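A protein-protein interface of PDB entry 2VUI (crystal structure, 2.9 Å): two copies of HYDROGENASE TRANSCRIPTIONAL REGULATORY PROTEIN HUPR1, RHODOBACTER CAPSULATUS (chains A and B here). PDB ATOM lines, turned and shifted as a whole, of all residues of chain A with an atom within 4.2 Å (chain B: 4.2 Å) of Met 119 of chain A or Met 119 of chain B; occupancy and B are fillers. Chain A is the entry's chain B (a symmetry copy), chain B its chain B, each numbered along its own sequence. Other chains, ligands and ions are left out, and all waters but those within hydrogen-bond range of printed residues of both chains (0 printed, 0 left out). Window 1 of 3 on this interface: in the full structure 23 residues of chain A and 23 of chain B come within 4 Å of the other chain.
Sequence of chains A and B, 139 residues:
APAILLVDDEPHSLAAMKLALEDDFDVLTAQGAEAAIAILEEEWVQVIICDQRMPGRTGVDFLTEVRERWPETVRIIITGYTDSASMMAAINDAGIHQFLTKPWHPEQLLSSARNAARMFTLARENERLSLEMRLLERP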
ATOM      1  N   VAL A  74     -12.743  22.358 -26.586  1.00  0.00           N
ATOM      2  CA  VAL A  74     -11.418  21.755 -26.414  1.00  0.00           C
ATOM      3  C   VAL A  74     -11.523  20.298 -25.969  1.00  0.00           C
ATOM      4  O   VAL A  74     -12.168  20.005 -24.964  1.00  0.00           O
ATOM      5  CB  VAL A  74     -10.535  22.558 -25.425  1.00  0.00           C
ATOM      6  CG1 VAL A  74      -9.174  21.905 -25.275  1.00  0.00           C
ATOM      7  CG2 VAL A  74     -10.393  23.988 -25.885  1.00  0.00           C
ATOM      8  N   ASN A 115      -6.273  25.101 -18.217  1.00  0.00           N
ATOM      9  CA  ASN A 115      -5.632  25.182 -19.517  1.00  0.00           C
ATOM     10  C   ASN A 115      -6.600  25.248 -20.667  1.00  0.00           C
ATOM     11  O   ASN A 115      -6.779  26.287 -21.308  1.00  0.00           O
ATOM     12  CB  ASN A 115      -4.783  23.936 -19.717  1.00  0.00           C
ATOM     13  CG  ASN A 115      -3.319  24.224 -19.598  1.00  0.00           C
ATOM     14  OD1 ASN A 115      -2.681  23.908 -18.577  1.00  0.00           O
ATOM     15  ND2 ASN A 115      -2.764  24.858 -20.643  1.00  0.00           N
ATOM     16  N   ALA A 116      -7.171  24.086 -20.948  1.00  0.00           N
ATOM     17  CA  ALA A 116      -8.255  23.945 -21.891  1.00  0.00           C
ATOM     18  C   ALA A 116      -9.162  25.177 -21.921  1.00  0.00           C
ATOM     19  O   ALA A 116      -9.382  25.752 -22.976  1.00  0.00           O
ATOM     20  CB  ALA A 116      -9.048  22.703 -21.560  1.00  0.00           C
ATOM     21  N   ALA A 117      -9.674  25.601 -20.772  1.00  0.00           N
ATOM     22  CA  ALA A 117     -10.623  26.711 -20.763  1.00  0.00           C
ATOM     23  C   ALA A 117      -9.994  28.057 -21.112  1.00  0.00           C
ATOM     24  O   ALA A 117     -10.654  28.923 -21.672  1.00  0.00           O
ATOM     25  CB  ALA A 117     -11.346  26.787 -19.446  1.00  0.00           C
ATOM     26  N   ARG A 118      -8.722  28.243 -20.776  1.00  0.00           N
ATOM     27  CA  ARG A 118      -8.026  29.454 -21.194  1.00  0.00           C
ATOM     28  C   ARG A 118      -7.815  29.380 -22.687  1.00  0.00           C
ATOM     29  O   ARG A 118      -8.034  30.350 -23.415  1.00  0.00           O
ATOM     30  CB  ARG A 118      -6.680  29.596 -20.496  1.00  0.00           C
ATOM     31  CG  ARG A 118      -6.685  30.556 -19.316  1.00  0.00           C
ATOM     32  CD  ARG A 118      -5.262  30.958 -18.949  1.00  0.00           C
ATOM     33  NE  ARG A 118      -4.369  29.811 -19.034  1.00  0.00           N
ATOM     34  CZ  ARG A 118      -4.135  28.970 -18.032  1.00  0.00           C
ATOM     35  NH1 ARG A 118      -4.716  29.162 -16.851  1.00  0.00           N
ATOM     36  NH2 ARG A 118      -3.318  27.934 -18.211  1.00  0.00           N
ATOM     37  N   MET A 119      -7.385  28.206 -23.129  1.00  0.00           N
ATOM     38  CA  MET A 119      -7.240  27.904 -24.545  1.00  0.00           C
ATOM     39  C   MET A 119      -8.532  28.095 -25.325  1.00  0.00           C
ATOM     40  O   MET A 119      -8.530  28.610 -26.443  1.00  0.00           O
ATOM     41  CB  MET A 119      -6.789  26.460 -24.711  1.00  0.00           C
ATOM     42  CG  MET A 119      -6.933  25.950 -26.118  1.00  0.00           C
ATOM     43  SD  MET A 119      -5.568  24.881 -26.580  1.00  0.00           S
ATOM     44  CE  MET A 119      -4.162  25.999 -26.322  1.00  0.00           C
ATOM     45  N   PHE A 120      -9.635  27.645 -24.742  1.00  0.00           N
ATOM     46  CA  PHE A 120     -10.909  27.666 -25.439  1.00  0.00           C
ATOM     47  C   PHE A 120     -11.231  29.111 -25.663  1.00  0.00           C
ATOM     48  O   PHE A 120     -11.813  29.496 -26.681  1.00  0.00           O
ATOM     49  CB  PHE A 120     -11.991  26.988 -24.599  1.00  0.00           C
ATOM     50  CG  PHE A 120     -13.361  27.572 -24.788  1.00  0.00           C
ATOM     51  CD1 PHE A 120     -14.211  27.085 -25.775  1.00  0.00           C
ATOM     52  CD2 PHE A 120     -13.806  28.600 -23.975  1.00  0.00           C
ATOM     53  CE1 PHE A 120     -15.480  27.615 -25.966  1.00  0.00           C
ATOM     54  CE2 PHE A 120     -15.068  29.130 -24.150  1.00  0.00           C
ATOM     55  CZ  PHE A 120     -15.911  28.635 -25.154  1.00  0.00           C
ATOM     56  N   THR A 121     -10.814  29.907 -24.688  1.00  0.00           N
ATOM     57  CA  THR A 121     -10.983  31.347 -24.707  1.00  0.00           C
ATOM     58  C   THR A 121     -10.134  32.050 -25.776  1.00  0.00           C
ATOM     59  O   THR A 121     -10.644  32.870 -26.536  1.00  0.00           O
ATOM     60  CB  THR A 121     -10.699  31.913 -23.316  1.00  0.00           C
ATOM     61  OG1 THR A 121     -11.940  32.070 -22.618  1.00  0.00           O
ATOM     62  CG2 THR A 121      -9.987  33.244 -23.411  1.00  0.00           C
ATOM     63  N   LEU A 122      -8.847  31.732 -25.844  1.00  0.00           N
ATOM     64  CA  LEU A 122      -8.006  32.277 -26.904  1.00  0.00           C
ATOM     65  C   LEU A 122      -8.609  31.977 -28.263  1.00  0.00           C
ATOM     66  O   LEU A 122      -8.986  32.873 -29.006  1.00  0.00           O
ATOM     67  CB  LEU A 122      -6.610  31.670 -26.859  1.00  0.00           C
ATOM     68  CG  LEU A 122      -5.566  32.357 -25.991  1.00  0.00           C
ATOM     69  CD1 LEU A 122      -4.192  31.992 -26.505  1.00  0.00           C
ATOM     70  CD2 LEU A 122      -5.774  33.857 -26.023  1.00  0.00           C
ATOM     71  N   ALA A 123      -8.677  30.692 -28.577  1.00  0.00           N
ATOM     72  CA  ALA A 123      -9.226  30.215 -29.836  1.00  0.00           C
ATOM     73  C   ALA A 123     -10.515  30.934 -30.216  1.00  0.00           C
ATOM     74  O   ALA A 123     -10.698  31.326 -31.374  1.00  0.00           O
ATOM     75  CB  ALA A 123      -9.458  28.701 -29.769  1.00  0.00           C
ATOM     76  N   VAL B  74       5.357  30.879 -22.897  1.00  0.00           N
ATOM     77  CA  VAL B  74       4.452  30.135 -22.017  1.00  0.00           C
ATOM     78  C   VAL B  74       5.204  29.516 -20.840  1.00  0.00           C
ATOM     79  O   VAL B  74       6.170  28.782 -21.042  1.00  0.00           O
ATOM     80  CB  VAL B  74       3.659  29.045 -22.782  1.00  0.00           C
ATOM     81  CG1 VAL B  74       2.734  28.299 -21.839  1.00  0.00           C
ATOM     82  CG2 VAL B  74       2.880  29.659 -23.919  1.00  0.00           C
ATOM     83  N   ASN B 115       1.008  21.330 -25.948  1.00  0.00           N
ATOM     84  CA  ASN B 115       0.040  22.298 -25.469  1.00  0.00           C
ATOM     85  C   ASN B 115       0.546  23.715 -25.478  1.00  0.00           C
ATOM     86  O   ASN B 115       0.143  24.545 -26.296  1.00  0.00           O
ATOM     87  CB  ASN B 115      -0.314  21.958 -24.029  1.00  0.00           C
ATOM     88  CG  ASN B 115      -1.683  21.364 -23.910  1.00  0.00           C
ATOM     89  OD1 ASN B 115      -1.842  20.143 -23.730  1.00  0.00           O
ATOM     90  ND2 ASN B 115      -2.704  22.227 -24.033  1.00  0.00           N
ATOM     91  N   ALA B 116       1.396  23.982 -24.498  1.00  0.00           N
ATOM     92  CA  ALA B 116       2.140  25.217 -24.409  1.00  0.00           C
ATOM     93  C   ALA B 116       2.485  25.786 -25.786  1.00  0.00           C
ATOM     94  O   ALA B 116       2.170  26.930 -26.074  1.00  0.00           O
ATOM     95  CB  ALA B 116       3.390  24.990 -23.592  1.00  0.00           C
ATOM     96  N   ALA B 117       3.112  24.994 -26.647  1.00  0.00           N
ATOM     97  CA  ALA B 117       3.551  25.522 -27.937  1.00  0.00           C
ATOM     98  C   ALA B 117       2.402  25.843 -28.889  1.00  0.00           C
ATOM     99  O   ALA B 117       2.512  26.745 -29.711  1.00  0.00           O
ATOM    100  CB  ALA B 117       4.539  24.594 -28.588  1.00  0.00           C
ATOM    101  N   ARG B 118       1.304  25.103 -28.793  1.00  0.00           N
ATOM    102  CA  ARG B 118       0.125  25.439 -29.584  1.00  0.00           C
ATOM    103  C   ARG B 118      -0.461  26.716 -29.030  1.00  0.00           C
ATOM    104  O   ARG B 118      -0.828  27.628 -29.772  1.00  0.00           O
ATOM    105  CB  ARG B 118      -0.921  24.333 -29.529  1.00  0.00           C
ATOM    106  CG  ARG B 118      -0.930  23.420 -30.745  1.00  0.00           C
ATOM    107  CD  ARG B 118      -2.234  22.634 -30.812  1.00  0.00           C
ATOM    108  NE  ARG B 118      -2.630  22.189 -29.483  1.00  0.00           N
ATOM    109  CZ  ARG B 118      -2.245  21.042 -28.932  1.00  0.00           C
ATOM    110  NH1 ARG B 118      -1.464  20.206 -29.610  1.00  0.00           N
ATOM    111  NH2 ARG B 118      -2.643  20.731 -27.700  1.00  0.00           N
ATOM    112  N   MET B 119      -0.539  26.762 -27.706  1.00  0.00           N
ATOM    113  CA  MET B 119      -0.961  27.953 -26.986  1.00  0.00           C
ATOM    114  C   MET B 119      -0.109  29.171 -27.306  1.00  0.00           C
ATOM    115  O   MET B 119      -0.617  30.281 -27.458  1.00  0.00           O
ATOM    116  CB  MET B 119      -0.881  27.694 -25.488  1.00  0.00           C
ATOM    117  CG  MET B 119      -0.969  28.946 -24.661  1.00  0.00           C
ATOM    118  SD  MET B 119      -1.920  28.688 -23.163  1.00  0.00           S
ATOM    119  CE  MET B 119      -3.501  28.130 -23.858  1.00  0.00           C
ATOM    120  N   PHE B 120       1.200  28.963 -27.375  1.00  0.00           N
ATOM    121  CA  PHE B 120       2.122  30.069 -27.559  1.00  0.00           C
ATOM    122  C   PHE B 120       1.817  30.639 -28.910  1.00  0.00           C
ATOM    123  O   PHE B 120       1.902  31.849 -29.138  1.00  0.00           O
ATOM    124  CB  PHE B 120       3.568  29.579 -27.487  1.00  0.00           C
ATOM    125  CG  PHE B 120       4.515  30.352 -28.358  1.00  0.00           C
ATOM    126  CD1 PHE B 120       5.165  31.482 -27.873  1.00  0.00           C
ATOM    127  CD2 PHE B 120       4.767  29.946 -29.657  1.00  0.00           C
ATOM    128  CE1 PHE B 120       6.042  32.212 -28.666  1.00  0.00           C
ATOM    129  CE2 PHE B 120       5.642  30.658 -30.452  1.00  0.00           C
ATOM    130  CZ  PHE B 120       6.284  31.800 -29.953  1.00  0.00           C
ATOM    131  N   THR B 121       1.435  29.731 -29.796  1.00  0.00           N
ATOM    132  CA  THR B 121       1.053  30.057 -31.158  1.00  0.00           C
ATOM    133  C   THR B 121      -0.261  30.846 -31.254  1.00  0.00           C
ATOM    134  O   THR B 121      -0.324  31.868 -31.934  1.00  0.00           O
ATOM    135  CB  THR B 121       0.992  28.778 -31.991  1.00  0.00           C
ATOM    136  OG1 THR B 121       2.233  28.619 -32.688  1.00  0.00           O
ATOM    137  CG2 THR B 121      -0.152  28.833 -32.979  1.00  0.00           C
ATOM    138  N   LEU B 122      -1.304  30.384 -30.576  1.00  0.00           N
ATOM    139  CA  LEU B 122      -2.550  31.141 -30.534  1.00  0.00           C
ATOM    140  C   LEU B 122      -2.294  32.553 -30.044  1.00  0.00           C
ATOM    141  O   LEU B 122      -2.499  33.524 -30.760  1.00  0.00           O
ATOM    142  CB  LEU B 122      -3.554  30.485 -29.593  1.00  0.00           C
ATOM    143  CG  LEU B 122      -4.483  29.428 -30.171  1.00  0.00           C
ATOM    144  CD1 LEU B 122      -5.714  29.335 -29.299  1.00  0.00           C
ATOM    145  CD2 LEU B 122      -4.854  29.791 -31.594  1.00  0.00           C
ATOM    146  N   ALA B 123      -1.855  32.645 -28.797  1.00  0.00           N
ATOM    147  CA  ALA B 123      -1.554  33.916 -28.159  1.00  0.00           C
ATOM    148  C   ALA B 123      -0.781  34.857 -29.076  1.00  0.00           C
ATOM    149  O   ALA B 123      -1.093  36.051 -29.156  1.00  0.00           O
ATOM    150  CB  ALA B 123      -0.776  33.679 -26.858  1.00  0.00           C
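Hydrophobic or aromatic side chains of chain B that line the printed part of chain A: Met 119, Leu 122 and Ala 123. Along chain B the printed residues that touch a printed residue of chain A span positions 119 to 123. Of the 10 printed residues of chain A, 3 touch a printed residue of chain B. Printed residues of chain A that touch a printed residue of chain B: Met 119, Leu 122 and Ala 123. Hydrophobic or aromatic side chains of chain A within 4 Å of the printed part of chain B: Met 119, Leu 122 and Ala 123. Among the printed residues, 4 pairs touch across the chains. Among the printed residues, no Asp or Glu carboxylate lies within 4 Å of a Lys or Arg side-chain nitrogen of the other chain.
Met 119 of chain B touches its own counterpart, Met 119 of chain A. Leu 122 of chain A touches its own counterpart, Leu 122 of chain B. Leu 122 of chain A touches Ala 123 of chain B, and with the chains exchanged Ala 123 of chain A touches Leu 122 of chain B. Positions printed for both chains: 74, 115, 116, 117, 118, 119, 120, 121, 122 and 123. Of the 4 pairs that touch across the chains among the printed residues, 4 have their exchanged pair printed and touching as well.
Met 119 of chain A touches just one residue of chain B: Met 119 (3.3 Å). Printed residues of chain B within 4 Å of Leu 122 of chain A: Leu 122 and Ala 123. Printed residues of chain B within 4 Å of Ala 123 of chain A: Leu 122 (3.3 Å). Of the printed residues of chain A, Ala 123 of chain B touches Leu 122. The nearest residue of chain B that does not touch Met 119 of chain A is Leu 122 of chain B (4.1 Å).
Among the printed residues, pairs that only touch across the chains: Met 119 of chain A with Met 119 of chain B, Leu 122 of chain A with Leu 122 of chain B, Leu 122 of chain A with Ala 123 of chain B and Ala 123 of chain A with Leu 122 of chain B.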
